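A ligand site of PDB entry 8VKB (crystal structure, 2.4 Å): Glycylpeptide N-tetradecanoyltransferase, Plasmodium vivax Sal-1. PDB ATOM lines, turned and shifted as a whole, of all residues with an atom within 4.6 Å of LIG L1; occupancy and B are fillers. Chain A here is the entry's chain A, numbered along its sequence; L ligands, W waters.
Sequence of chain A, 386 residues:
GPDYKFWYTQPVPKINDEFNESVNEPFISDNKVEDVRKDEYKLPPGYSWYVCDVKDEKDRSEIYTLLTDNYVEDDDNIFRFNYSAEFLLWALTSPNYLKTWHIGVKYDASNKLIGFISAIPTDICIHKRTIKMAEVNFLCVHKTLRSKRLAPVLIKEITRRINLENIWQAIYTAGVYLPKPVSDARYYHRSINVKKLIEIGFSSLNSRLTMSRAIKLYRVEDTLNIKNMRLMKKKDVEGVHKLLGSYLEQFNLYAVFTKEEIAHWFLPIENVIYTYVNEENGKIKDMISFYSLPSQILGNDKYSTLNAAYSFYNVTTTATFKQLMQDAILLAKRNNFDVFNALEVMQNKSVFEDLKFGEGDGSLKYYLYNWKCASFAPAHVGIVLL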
ATOM      1  N   VAL A  72      22.889   4.472   0.973  1.00  0.00           N
ATOM      2  CA  VAL A  72      21.987   3.409   0.547  1.00  0.00           C
ATOM      3  C   VAL A  72      22.038   3.233  -0.962  1.00  0.00           C
ATOM      4  O   VAL A  72      22.118   4.209  -1.722  1.00  0.00           O
ATOM      5  CB  VAL A  72      20.543   3.704   1.009  1.00  0.00           C
ATOM      6  CG1 VAL A  72      19.645   2.502   0.757  1.00  0.00           C
ATOM      7  CG2 VAL A  72      20.509   4.094   2.470  1.00  0.00           C
ATOM      8  N   GLU A  73      21.980   1.975  -1.403  1.00  0.00           N
ATOM      9  CA  GLU A  73      21.875   1.634  -2.806  1.00  0.00           C
ATOM     10  C   GLU A  73      20.571   0.878  -3.043  1.00  0.00           C
ATOM     11  O   GLU A  73      19.992   0.291  -2.124  1.00  0.00           O
ATOM     12  CB  GLU A  73      23.067   0.769  -3.266  1.00  0.00           C
ATOM     13  CG  GLU A  73      24.425   1.398  -3.004  1.00  0.00           C
ATOM     14  CD  GLU A  73      25.559   0.616  -3.633  1.00  0.00           C
ATOM     15  OE1 GLU A  73      25.276  -0.368  -4.355  1.00  0.00           O
ATOM     16  OE2 GLU A  73      26.733   0.983  -3.421  1.00  0.00           O
ATOM     17  N   ASP A  74      20.103   0.917  -4.284  1.00  0.00           N
ATOM     18  CA  ASP A  74      18.897   0.178  -4.630  1.00  0.00           C
ATOM     19  C   ASP A  74      19.192  -1.317  -4.704  1.00  0.00           C
ATOM     20  O   ASP A  74      20.347  -1.757  -4.628  1.00  0.00           O
ATOM     21  CB  ASP A  74      18.332   0.673  -5.955  1.00  0.00           C
ATOM     22  CG  ASP A  74      19.245   0.368  -7.125  1.00  0.00           C
ATOM     23  OD1 ASP A  74      20.458   0.629  -7.021  1.00  0.00           O
ATOM     24  OD2 ASP A  74      18.744  -0.155  -8.147  1.00  0.00           O
ATOM     25  N   PHE A  79      21.749   2.716  -8.364  1.00  0.00           N
ATOM     26  CA  PHE A  79      21.570   4.022  -7.728  1.00  0.00           C
ATOM     27  C   PHE A  79      22.229   4.018  -6.360  1.00  0.00           C
ATOM     28  O   PHE A  79      22.246   2.993  -5.660  1.00  0.00           O
ATOM     29  CB  PHE A  79      20.088   4.367  -7.573  1.00  0.00           C
ATOM     30  CG  PHE A  79      19.358   4.570  -8.869  1.00  0.00           C
ATOM     31  CD1 PHE A  79      19.900   5.346  -9.876  1.00  0.00           C
ATOM     32  CD2 PHE A  79      18.116   3.985  -9.074  1.00  0.00           C
ATOM     33  CE1 PHE A  79      19.226   5.528 -11.069  1.00  0.00           C
ATOM     34  CE2 PHE A  79      17.442   4.166 -10.268  1.00  0.00           C
ATOM     35  CZ  PHE A  79      17.999   4.940 -11.257  1.00  0.00           C
ATOM     36  N   ARG A  80      22.772   5.168  -5.984  1.00  0.00           N
ATOM     37  CA  ARG A  80      23.182   5.435  -4.613  1.00  0.00           C
ATOM     38  C   ARG A  80      22.773   6.860  -4.260  1.00  0.00           C
ATOM     39  O   ARG A  80      23.051   7.792  -5.028  1.00  0.00           O
ATOM     40  CB  ARG A  80      24.690   5.252  -4.418  1.00  0.00           C
ATOM     41  CG  ARG A  80      25.132   5.483  -2.968  1.00  0.00           C
ATOM     42  CD  ARG A  80      26.642   5.382  -2.798  1.00  0.00           C
ATOM     43  NE  ARG A  80      27.163   4.080  -3.202  1.00  0.00           N
ATOM     44  CZ  ARG A  80      28.029   3.874  -4.194  1.00  0.00           C
ATOM     45  NH1 ARG A  80      28.547   4.878  -4.881  1.00  0.00           N
ATOM     46  NH2 ARG A  80      28.388   2.629  -4.489  1.00  0.00           N
ATOM     47  N   PHE A  81      22.120   7.031  -3.123  1.00  0.00           N
ATOM     48  CA  PHE A  81      21.685   8.351  -2.706  1.00  0.00           C
ATOM     49  C   PHE A  81      22.868   9.302  -2.637  1.00  0.00           C
ATOM     50  O   PHE A  81      23.967   8.933  -2.199  1.00  0.00           O
ATOM     51  CB  PHE A  81      20.989   8.281  -1.340  1.00  0.00           C
ATOM     52  CG  PHE A  81      19.585   7.714  -1.395  1.00  0.00           C
ATOM     53  CD1 PHE A  81      18.753   7.956  -2.494  1.00  0.00           C
ATOM     54  CD2 PHE A  81      19.101   6.939  -0.355  1.00  0.00           C
ATOM     55  CE1 PHE A  81      17.476   7.432  -2.543  1.00  0.00           C
ATOM     56  CE2 PHE A  81      17.817   6.418  -0.397  1.00  0.00           C
ATOM     57  CZ  PHE A  81      17.002   6.661  -1.492  1.00  0.00           C
ATOM     58  N   TYR A  83      22.914  12.796  -1.202  1.00  0.00           N
ATOM     59  CA  TYR A  83      22.518  13.987  -0.467  1.00  0.00           C
ATOM     60  C   TYR A  83      23.545  15.096  -0.672  1.00  0.00           C
ATOM     61  O   TYR A  83      24.748  14.873  -0.533  1.00  0.00           O
ATOM     62  CB  TYR A  83      22.390  13.675   1.033  1.00  0.00           C
ATOM     63  CG  TYR A  83      21.161  12.870   1.406  1.00  0.00           C
ATOM     64  CD1 TYR A  83      19.936  13.487   1.598  1.00  0.00           C
ATOM     65  CD2 TYR A  83      21.239  11.489   1.578  1.00  0.00           C
ATOM     66  CE1 TYR A  83      18.815  12.748   1.950  1.00  0.00           C
ATOM     67  CE2 TYR A  83      20.131  10.756   1.926  1.00  0.00           C
ATOM     68  CZ  TYR A  83      18.914  11.384   2.107  1.00  0.00           C
ATOM     69  OH  TYR A  83      17.809  10.646   2.463  1.00  0.00           O
ATOM     70  N   ASN A 137      18.734   9.393  11.719  1.00  0.00           N
ATOM     71  CA  ASN A 137      18.881   9.322  10.269  1.00  0.00           C
ATOM     72  C   ASN A 137      20.368   9.322   9.934  1.00  0.00           C
ATOM     73  O   ASN A 137      21.212   9.672  10.766  1.00  0.00           O
ATOM     74  CB  ASN A 137      18.174  10.497   9.589  1.00  0.00           C
ATOM     75  CG  ASN A 137      17.652  10.155   8.207  1.00  0.00           C
ATOM     76  OD1 ASN A 137      18.186   9.274   7.532  1.00  0.00           O
ATOM     77  ND2 ASN A 137      16.604  10.852   7.786  1.00  0.00           N
ATOM     78  N   THR A 173      13.125   5.441  10.278  1.00  0.00           N
ATOM     79  CA  THR A 173      12.624   4.643   9.173  1.00  0.00           C
ATOM     80  C   THR A 173      13.783   3.887   8.533  1.00  0.00           C
ATOM     81  O   THR A 173      14.952   4.242   8.682  1.00  0.00           O
ATOM     82  CB  THR A 173      11.928   5.498   8.111  1.00  0.00           C
ATOM     83  OG1 THR A 173      12.831   6.493   7.616  1.00  0.00           O
ATOM     84  CG2 THR A 173      10.684   6.179   8.693  1.00  0.00           C
ATOM     85  N   GLY A 175      14.381   0.862   4.990  1.00  0.00           N
ATOM     86  CA  GLY A 175      13.848  -0.061   4.012  1.00  0.00           C
ATOM     87  C   GLY A 175      13.971  -1.515   4.411  1.00  0.00           C
ATOM     88  O   GLY A 175      13.211  -2.353   3.905  1.00  0.00           O
ATOM     89  N   TYR A 187       6.310   2.565  -1.580  1.00  0.00           N
ATOM     90  CA  TYR A 187       6.623   3.815  -2.270  1.00  0.00           C
ATOM     91  C   TYR A 187       6.345   3.686  -3.766  1.00  0.00           C
ATOM     92  O   TYR A 187       6.376   2.589  -4.328  1.00  0.00           O
ATOM     93  CB  TYR A 187       8.080   4.239  -2.047  1.00  0.00           C
ATOM     94  CG  TYR A 187       9.094   3.120  -2.056  1.00  0.00           C
ATOM     95  CD1 TYR A 187       9.539   2.567  -3.247  1.00  0.00           C
ATOM     96  CD2 TYR A 187       9.619   2.629  -0.872  1.00  0.00           C
ATOM     97  CE1 TYR A 187      10.472   1.545  -3.255  1.00  0.00           C
ATOM     98  CE2 TYR A 187      10.554   1.611  -0.864  1.00  0.00           C
ATOM     99  CZ  TYR A 187      10.970   1.079  -2.062  1.00  0.00           C
ATOM    100  OH  TYR A 187      11.900   0.067  -2.061  1.00  0.00           O
ATOM    101  N   TYR A 188       6.059   4.819  -4.389  1.00  0.00           N
ATOM    102  CA  TYR A 188       5.707   4.886  -5.799  1.00  0.00           C
ATOM    103  C   TYR A 188       6.525   5.986  -6.471  1.00  0.00           C
ATOM    104  O   TYR A 188       7.079   6.865  -5.810  1.00  0.00           O
ATOM    105  CB  TYR A 188       4.204   5.160  -5.985  1.00  0.00           C
ATOM    106  CG  TYR A 188       3.299   4.069  -5.462  1.00  0.00           C
ATOM    107  CD1 TYR A 188       3.165   3.858  -4.094  1.00  0.00           C
ATOM    108  CD2 TYR A 188       2.584   3.264  -6.329  1.00  0.00           C
ATOM    109  CE1 TYR A 188       2.329   2.864  -3.615  1.00  0.00           C
ATOM    110  CE2 TYR A 188       1.748   2.256  -5.846  1.00  0.00           C
ATOM    111  CZ  TYR A 188       1.631   2.073  -4.483  1.00  0.00           C
ATOM    112  OH  TYR A 188       0.813   1.079  -4.000  1.00  0.00           O
ATOM    113  N   PHE A 202      15.757   2.189 -15.763  1.00  0.00           N
ATOM    114  CA  PHE A 202      14.791   2.120 -14.658  1.00  0.00           C
ATOM    115  C   PHE A 202      13.397   1.777 -15.175  1.00  0.00           C
ATOM    116  O   PHE A 202      12.713   0.927 -14.601  1.00  0.00           O
ATOM    117  CB  PHE A 202      14.773   3.440 -13.891  1.00  0.00           C
ATOM    118  CG  PHE A 202      13.898   3.420 -12.667  1.00  0.00           C
ATOM    119  CD1 PHE A 202      14.201   2.603 -11.600  1.00  0.00           C
ATOM    120  CD2 PHE A 202      12.762   4.212 -12.600  1.00  0.00           C
ATOM    121  CE1 PHE A 202      13.405   2.583 -10.472  1.00  0.00           C
ATOM    122  CE2 PHE A 202      11.962   4.198 -11.480  1.00  0.00           C
ATOM    123  CZ  PHE A 202      12.277   3.373 -10.412  1.00  0.00           C
ATOM    124  N   SER A 295      20.073  10.694  -6.934  1.00  0.00           N
ATOM    125  CA  SER A 295      20.647   9.351  -6.877  1.00  0.00           C
ATOM    126  C   SER A 295      21.741   9.253  -7.938  1.00  0.00           C
ATOM    127  O   SER A 295      21.456   9.310  -9.130  1.00  0.00           O
ATOM    128  CB  SER A 295      19.578   8.278  -7.102  1.00  0.00           C
ATOM    129  OG  SER A 295      18.749   8.137  -5.958  1.00  0.00           O
ATOM    130  N   LEU A 306      20.415  11.056 -10.990  1.00  0.00           N
ATOM    131  CA  LEU A 306      18.991  11.084 -11.302  1.00  0.00           C
ATOM    132  C   LEU A 306      18.329  12.038 -10.315  1.00  0.00           C
ATOM    133  O   LEU A 306      18.152  11.703  -9.142  1.00  0.00           O
ATOM    134  CB  LEU A 306      18.372   9.685 -11.206  1.00  0.00           C
ATOM    135  CG  LEU A 306      16.879   9.616 -11.474  1.00  0.00           C
ATOM    136  CD1 LEU A 306      16.584   9.823 -12.958  1.00  0.00           C
ATOM    137  CD2 LEU A 306      16.287   8.303 -10.989  1.00  0.00           C
ATOM    138  N   ALA A 308      15.775  13.365  -8.379  1.00  0.00           N
ATOM    139  CA  ALA A 308      14.470  12.928  -7.915  1.00  0.00           C
ATOM    140  C   ALA A 308      13.890  13.923  -6.909  1.00  0.00           C
ATOM    141  O   ALA A 308      14.614  14.547  -6.129  1.00  0.00           O
ATOM    142  CB  ALA A 308      14.551  11.545  -7.276  1.00  0.00           C
ATOM    143  N   TYR A 310      10.879  14.215  -3.866  1.00  0.00           N
ATOM    144  CA  TYR A 310      10.141  13.385  -2.926  1.00  0.00           C
ATOM    145  C   TYR A 310       9.031  14.208  -2.283  1.00  0.00           C
ATOM    146  O   TYR A 310       9.293  15.268  -1.702  1.00  0.00           O
ATOM    147  CB  TYR A 310      11.073  12.791  -1.865  1.00  0.00           C
ATOM    148  CG  TYR A 310      11.984  11.721  -2.408  1.00  0.00           C
ATOM    149  CD1 TYR A 310      13.104  12.050  -3.173  1.00  0.00           C
ATOM    150  CD2 TYR A 310      11.735  10.379  -2.173  1.00  0.00           C
ATOM    151  CE1 TYR A 310      13.943  11.082  -3.676  1.00  0.00           C
ATOM    152  CE2 TYR A 310      12.569   9.389  -2.675  1.00  0.00           C
ATOM    153  CZ  TYR A 310      13.667   9.751  -3.429  1.00  0.00           C
ATOM    154  OH  TYR A 310      14.499   8.785  -3.926  1.00  0.00           O
ATOM    155  N   VAL A 339      11.938  12.824 -11.795  1.00  0.00           N
ATOM    156  CA  VAL A 339      10.938  11.888 -11.304  1.00  0.00           C
ATOM    157  C   VAL A 339      10.354  12.438 -10.009  1.00  0.00           C
ATOM    158  O   VAL A 339      11.003  13.219  -9.301  1.00  0.00           O
ATOM    159  CB  VAL A 339      11.538  10.476 -11.104  1.00  0.00           C
ATOM    160  CG1 VAL A 339      12.668  10.510 -10.078  1.00  0.00           C
ATOM    161  CG2 VAL A 339      10.464   9.480 -10.695  1.00  0.00           C
ATOM    162  N   ASN A 341       8.551  11.058  -6.486  1.00  0.00           N
ATOM    163  CA  ASN A 341       8.329   9.885  -5.655  1.00  0.00           C
ATOM    164  C   ASN A 341       7.500  10.250  -4.424  1.00  0.00           C
ATOM    165  O   ASN A 341       7.563  11.372  -3.919  1.00  0.00           O
ATOM    166  CB  ASN A 341       9.661   9.273  -5.201  1.00  0.00           C
ATOM    167  CG  ASN A 341      10.511   8.800  -6.373  1.00  0.00           C
ATOM    168  OD1 ASN A 341      10.001   8.565  -7.467  1.00  0.00           O
ATOM    169  ND2 ASN A 341      11.809   8.655  -6.137  1.00  0.00           N
ATOM    170  N   ALA A 342       6.719   9.275  -3.952  1.00  0.00           N
ATOM    171  CA  ALA A 342       5.865   9.486  -2.793  1.00  0.00           C
ATOM    172  C   ALA A 342       5.559   8.136  -2.141  1.00  0.00           C
ATOM    173  O   ALA A 342       5.772   7.077  -2.739  1.00  0.00           O
ATOM    174  CB  ALA A 342       4.563  10.190  -3.181  1.00  0.00           C
ATOM    175  N   LEU A 343       5.080   8.206  -0.913  1.00  0.00           N
ATOM    176  CA  LEU A 343       4.661   7.030  -0.152  1.00  0.00           C
ATOM    177  C   LEU A 343       3.143   6.931  -0.128  1.00  0.00           C
ATOM    178  O   LEU A 343       2.420   7.863  -0.486  1.00  0.00           O
ATOM    179  CB  LEU A 343       5.208   7.093   1.285  1.00  0.00           C
ATOM    180  CG  LEU A 343       6.725   7.017   1.441  1.00  0.00           C
ATOM    181  CD1 LEU A 343       7.140   7.495   2.828  1.00  0.00           C
ATOM    182  CD2 LEU A 343       7.222   5.595   1.203  1.00  0.00           C
ATOM    183  N   LEU A 364       8.895   1.233   2.860  1.00  0.00           N
ATOM    184  CA  LEU A 364       9.584   1.958   3.925  1.00  0.00           C
ATOM    185  C   LEU A 364       8.860   1.718   5.235  1.00  0.00           C
ATOM    186  O   LEU A 364       7.649   1.958   5.329  1.00  0.00           O
ATOM    187  CB  LEU A 364       9.654   3.449   3.610  1.00  0.00           C
ATOM    188  CG  LEU A 364      10.743   4.242   4.333  1.00  0.00           C
ATOM    189  CD1 LEU A 364      12.100   3.968   3.688  1.00  0.00           C
ATOM    190  CD2 LEU A 364      10.440   5.731   4.336  1.00  0.00           C
ATOM    191  N   LEU A 385       9.869  11.364   6.852  1.00  0.00           N
ATOM    192  CA  LEU A 385      11.246  11.590   7.248  1.00  0.00           C
ATOM    193  C   LEU A 385      12.135  11.726   6.019  1.00  0.00           C
ATOM    194  O   LEU A 385      11.857  11.157   4.955  1.00  0.00           O
ATOM    195  CB  LEU A 385      11.762  10.456   8.131  1.00  0.00           C
ATOM    196  CG  LEU A 385      11.569  10.633   9.634  1.00  0.00           C
ATOM    197  CD1 LEU A 385      10.153  11.073   9.989  1.00  0.00           C
ATOM    198  CD2 LEU A 385      11.925   9.336  10.356  1.00  0.00           C
ATOM    199  N   LEU A 386      13.220  12.484   6.176  1.00  0.00           N
ATOM    200  CA  LEU A 386      14.135  12.754   5.074  1.00  0.00           C
ATOM    201  C   LEU A 386      14.964  11.523   4.704  1.00  0.00           C
ATOM    202  O   LEU A 386      15.172  10.629   5.534  1.00  0.00           O
ATOM    203  CB  LEU A 386      15.066  13.911   5.425  1.00  0.00           C
ATOM    204  CG  LEU A 386      14.387  15.144   6.011  1.00  0.00           C
ATOM    205  CD1 LEU A 386      15.430  16.210   6.332  1.00  0.00           C
ATOM    206  CD2 LEU A 386      13.319  15.689   5.073  1.00  0.00           C
ATOM    207  OXT LEU A 386      15.447  11.387   3.580  1.00  0.00           O
HETATM  208  C1  LIG L   1      13.539   6.835  -8.914  1.00  0.00           C
HETATM  209  C2  LIG L   1      13.964   5.508  -8.290  1.00  0.00           C
HETATM  210  C3  LIG L   1      16.446   3.424  -4.500  1.00  0.00           C
HETATM  211  C4  LIG L   1      15.279   2.488  -4.169  1.00  0.00           C
HETATM  212  C5  LIG L   1      13.923   3.216  -4.132  1.00  0.00           C
HETATM  213  C6  LIG L   1      10.836   5.990  -3.569  1.00  0.00           C
HETATM  214  C7  LIG L   1      10.592   6.514  -2.264  1.00  0.00           C
HETATM  215  C8  LIG L   1       9.495   7.391  -2.057  1.00  0.00           C
HETATM  216  C9  LIG L   1       9.247   7.919  -0.789  1.00  0.00           C
HETATM  217  C10 LIG L   1      10.081   7.570   0.269  1.00  0.00           C
HETATM  218  C11 LIG L   1      11.164   6.710   0.071  1.00  0.00           C
HETATM  219  C12 LIG L   1      17.870   3.046  -2.361  1.00  0.00           C
HETATM  220  C13 LIG L   1      17.556   3.662  -3.732  1.00  0.00           C
HETATM  221  C14 LIG L   1      19.588   5.040  -3.916  1.00  0.00           C
HETATM  222  C15 LIG L   1      16.571   4.187  -5.652  1.00  0.00           C
HETATM  223  C16 LIG L   1      15.562   4.233  -6.797  1.00  0.00           C
HETATM  224  C17 LIG L   1      15.140   6.747  -6.557  1.00  0.00           C
HETATM  225  C18 LIG L   1      15.068   7.933  -7.509  1.00  0.00           C
HETATM  226  C19 LIG L   1      12.753   4.779  -2.739  1.00  0.00           C
HETATM  227  C20 LIG L   1      11.900   5.138  -3.791  1.00  0.00           C
HETATM  228  C21 LIG L   1      11.419   6.178  -1.234  1.00  0.00           C
HETATM  229  C22 LIG L   1      12.522   5.294  -1.463  1.00  0.00           C
HETATM  230  C23 LIG L   1      13.456   4.883  -0.334  1.00  0.00           C
HETATM  231  C24 LIG L   1      14.170   5.825   0.396  1.00  0.00           C
HETATM  232  C25 LIG L   1      15.003   5.404   1.414  1.00  0.00           C
HETATM  233  C26 LIG L   1      16.625   5.990   3.333  1.00  0.00           C
HETATM  234  C27 LIG L   1      15.949   6.154   4.694  1.00  0.00           C
HETATM  235  C28 LIG L   1      14.563   7.900   3.834  1.00  0.00           C
HETATM  236  C29 LIG L   1      15.217   7.754   2.459  1.00  0.00           C
HETATM  237  C30 LIG L   1      14.481   3.209   1.021  1.00  0.00           C
HETATM  238  C31 LIG L   1      13.625   3.537  -0.010  1.00  0.00           C
HETATM  239  N1  LIG L   1      18.303   4.527  -4.379  1.00  0.00           N
HETATM  240  N2  LIG L   1      17.706   4.860  -5.580  1.00  0.00           N
HETATM  241  N3  LIG L   1      14.905   5.484  -7.197  1.00  0.00           N
HETATM  242  N4  LIG L   1      15.754   6.394   2.185  1.00  0.00           N
HETATM  243  N5  LIG L   1      15.358   7.422   4.905  1.00  0.00           N
HETATM  244  N6  LIG L   1      15.147   4.123   1.705  1.00  0.00           N
HETATM  245  O1  LIG L   1      13.832   7.997  -8.161  1.00  0.00           O
HETATM  246  O2  LIG L   1      15.315   3.238  -7.381  1.00  0.00           O
HETATM  247  O3  LIG L   1      13.851   3.917  -2.920  1.00  0.00           O
HETATM  248  S1  LG2 L   2      18.030   4.041   7.588  1.00  0.00           S
HETATM  249  C1  LG2 L   2      19.315   3.572   6.258  1.00  0.00           C
HETATM  250  C2  LG2 L   2      20.673   3.165   6.879  1.00  0.00           C
HETATM  251  N1  LG2 L   2      21.875   3.449   6.068  1.00  0.00           N
HETATM  252  C3  LG2 L   2      22.368   2.620   5.019  1.00  0.00           C
HETATM  253  O1  LG2 L   2      21.745   1.606   4.771  1.00  0.00           O
HETATM  254  C4  LG2 L   2      23.624   2.921   4.170  1.00  0.00           C
HETATM  255  C5  LG2 L   2      24.350   1.710   3.584  1.00  0.00           C
HETATM  256  N2  LG2 L   2      24.561   0.629   4.554  1.00  0.00           N
HETATM  257  C6  LG2 L   2      25.338   0.735   5.728  1.00  0.00           C
HETATM  258  O2  LG2 L   2      25.897   1.804   5.932  1.00  0.00           O
HETATM  259  C7  LG2 L   2      25.521  -0.456   6.745  1.00  0.00           C
HETATM  260  O3  LG2 L   2      25.182  -1.610   6.045  1.00  0.00           O
HETATM  261  C8  LG2 L   2      24.626  -0.289   8.026  1.00  0.00           C
HETATM  262  C9  LG2 L   2      24.728  -1.618   8.949  1.00  0.00           C
HETATM  263  C10 LG2 L   2      23.172  -0.074   7.620  1.00  0.00           C
HETATM  264  C11 LG2 L   2      25.113   0.935   8.825  1.00  0.00           C
HETATM  265  N3  LG2 L   2      18.820   0.498  10.860  1.00  0.00           N
HETATM  266  O4  LG2 L   2      27.303  -3.184  11.876  1.00  0.00           O
HETATM  267  P1  LG2 L   2      26.793  -4.515  11.439  1.00  0.00           P
HETATM  268  C12 LG2 L   2      21.328  -3.931  12.266  1.00  0.00           C
HETATM  269  C13 LG2 L   2      19.022  -0.108  12.086  1.00  0.00           C
HETATM  270  O5  LG2 L   2      27.700  -5.703  11.393  1.00  0.00           O
HETATM  271  P2  LG2 L   2      26.600  -3.425   8.711  1.00  0.00           P
HETATM  272  C14 LG2 L   2      18.676   5.285   8.809  1.00  0.00           C
HETATM  273  O6  LG2 L   2      19.483   6.107   8.445  1.00  0.00           O
HETATM  274  C15 LG2 L   2      21.051  -5.398  11.953  1.00  0.00           C
HETATM  275  O7  LG2 L   2      19.765  -5.699  12.380  1.00  0.00           O
HETATM  276  N4  LG2 L   2      19.687  -1.246  12.367  1.00  0.00           N
HETATM  277  O8  LG2 L   2      26.269  -4.355   9.958  1.00  0.00           O
HETATM  278  C16 LG2 L   2      18.193   5.271  10.275  1.00  0.00           C
HETATM  279  C17 LG2 L   2      22.034  -6.104  12.937  1.00  0.00           C
HETATM  280  O9  LG2 L   2      21.439  -6.322  14.108  1.00  0.00           O
HETATM  281  P3  LG2 L   2      20.997  -7.752  14.632  1.00  0.00           P
HETATM  282  C18 LG2 L   2      20.210  -1.869  11.241  1.00  0.00           C
HETATM  283  O10 LG2 L   2      25.801  -3.799   7.503  1.00  0.00           O
HETATM  284  C19 LG2 L   2      18.681   4.093  11.156  1.00  0.00           C
HETATM  285  C20 LG2 L   2      23.250  -5.061  12.969  1.00  0.00           C
HETATM  286  O11 LG2 L   2      22.726  -3.821  12.444  1.00  0.00           O
HETATM  287  C21 LG2 L   2      20.058  -1.340   9.910  1.00  0.00           C
HETATM  288  O12 LG2 L   2      28.023  -3.052   8.462  1.00  0.00           O
HETATM  289  C22 LG2 L   2      18.239   4.107  12.645  1.00  0.00           C
HETATM  290  C23 LG2 L   2      24.475  -5.525  12.125  1.00  0.00           C
HETATM  291  O13 LG2 L   2      25.664  -4.892  12.487  1.00  0.00           O
HETATM  292  C24 LG2 L   2      19.338  -0.132   9.762  1.00  0.00           C
HETATM  293  N5  LG2 L   2      19.141   0.454   8.517  1.00  0.00           N
HETATM  294  O14 LG2 L   2      26.016  -1.998   9.111  1.00  0.00           O
HETATM  295  C25 LG2 L   2      19.047   3.199  13.634  1.00  0.00           C
HETATM  296  N6  LG2 L   2      20.705  -2.217   9.006  1.00  0.00           N
HETATM  297  O15 LG2 L   2      20.182  -7.486  15.879  1.00  0.00           O
HETATM  298  C26 LG2 L   2      18.277   2.733  14.902  1.00  0.00           C
HETATM  299  C27 LG2 L   2      21.214  -3.207   9.774  1.00  0.00           C
HETATM  300  O16 LG2 L   2      20.222  -8.287  13.456  1.00  0.00           O
HETATM  301  C28 LG2 L   2      18.196   3.777  16.056  1.00  0.00           C
HETATM  302  N7  LG2 L   2      20.929  -3.030  11.127  1.00  0.00           N
HETATM  303  O17 LG2 L   2      22.359  -8.371  14.890  1.00  0.00           O
HETATM  304  C29 LG2 L   2      17.427   3.367  17.337  1.00  0.00           C
HETATM  305  C30 LG2 L   2      17.162   4.509  18.360  1.00  0.00           C
HETATM  306  C31 LG2 L   2      18.416   5.211  18.960  1.00  0.00           C
HETATM  307  C32 LG2 L   2      18.145   6.454  19.851  1.00  0.00           C
HETATM  308  C33 LG2 L   2      17.257   6.199  21.103  1.00  0.00           C
HETATM  309  C34 LG2 L   2      16.947   7.446  21.980  1.00  0.00           C
HETATM  310  C35 LG2 L   2      15.804   7.273  22.994  1.00  0.00           C
HETATM  311  O   HOH W   1       8.208  11.100  -0.224  1.00  0.00           O
HETATM  312  O   HOH W   2      13.664   9.366   0.169  1.00  0.00           O
HETATM  313  O   HOH W   3      10.403  10.492   1.410  1.00  0.00           O
HETATM  314  O   HOH W   4      16.878   9.648  -5.377  1.00  0.00           O
HETATM  315  O   HOH W   5      17.889   8.850   4.668  1.00  0.00           O
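O of Val 72 touches C14 of LIG L1, at 3.5 Å. O of Glu 73 touches C12 of LIG L1, 3.5 Å away. Asp 74 touches LIG L1 (N to C12, 3.6 Å). CB of Phe 79 touches N2 of LIG L1, at 3.1 Å. Arg 80 touches LIG L1 (CA to C14, 3.7 Å). CE2 of Phe 81 touches N4 of LIG L1, 3.3 Å away. OH of Tyr 83 touches C29 of LIG L1 (3.9 Å). Thr 173 touches LIG L1 (OG1 to N5, 3.8 Å). CB of Tyr 187 touches C7 of LIG L1, 3.4 Å away. Phe 202 touches LIG L1. CD2 of Leu 306 touches C18 of LIG L1 (3.7 Å). CB of Ala 308 touches C18 of LIG L1, at 3.7 Å. Tyr 310 touches LIG L1. Val 339 touches LIG L1 (CG1 to O1, 3.4 Å). Ala 342 touches LIG L1 (O to C8, 3.8 Å). Leu 343 touches LIG L1. Leu 364 touches LIG L1. Hydrophobic or aromatic side chains that line LIG L1: Val 72, Phe 79, Phe 81, Tyr 187, Phe 202, Leu 306, Ala 308, Tyr 310, Val 339, Leu 343 and Leu 364. 20 residues have an atom within 4 Å of LIG L1: Val 72, Glu 73, Asp 74, Phe 79, Arg 80, Phe 81, Tyr 83, Thr 173, Tyr 187, Phe 202, Ser 295, Leu 306, Ala 308, Tyr 310, Val 339, Asn 341, Ala 342, Leu 343, Leu 364 and Leu 386. The nearest printed residue that does not touch LIG L1 is Asn 137 (4.3 Å).
ND2 of Asn 341 is in hydrogen-bond range of O1 of LIG L1 (2.9 Å). The chain-end carboxylate (O) of Leu 386 lies within salt-bridge range of a nitrogen (N5) of LIG L1 (3.3 Å). OG of Ser 295 sits at hydrogen-bond distance from N2 of LIG L1 (3.5 Å).
Water W5 lies within hydrogen-bond range of OH of Tyr 83 (2.8 Å), OD1 of Asn 137 (2.9 Å), N5 of LIG L1 (2.9 Å) and O of Leu 386 (3.4 Å). Water W4 bridges OG of Ser 295 and OH of Tyr 310.
ND2 of Asn 341 lies close to OH of Tyr 310 (3.5 Å). The backbone NH (N) of Phe 79 sits at hydrogen-bond distance from the side-chain carboxylate (OD1) of Asp 74. The side-chain hydroxyl (OH) of Tyr 83 sits at hydrogen-bond distance from the chain-end carboxylate (OXT) of Leu 386, 2.7 Å away. The chain-end carboxylate (O) of Leu 386 lies within hydrogen-bond range of the side-chain amide nitrogen (ND2) of Asn 137 (2.7 Å). The backbone NH (N) of Phe 81 lies within hydrogen-bond range of the backbone carbonyl oxygen (O) of Val 72, at 3.2 Å. N of Leu 306 is in hydrogen-bond range of O of Ser 295, at 2.8 Å. The side-chain carboxylate (OE2) of Glu 73 is in salt-bridge range of the guanidinium group (NH2) of Arg 80, at 2.6 Å. The backbone carbonyl oxygen (O) of Ala 342 sits at hydrogen-bond distance from the backbone NH (N) of Tyr 188 (2.8 Å).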
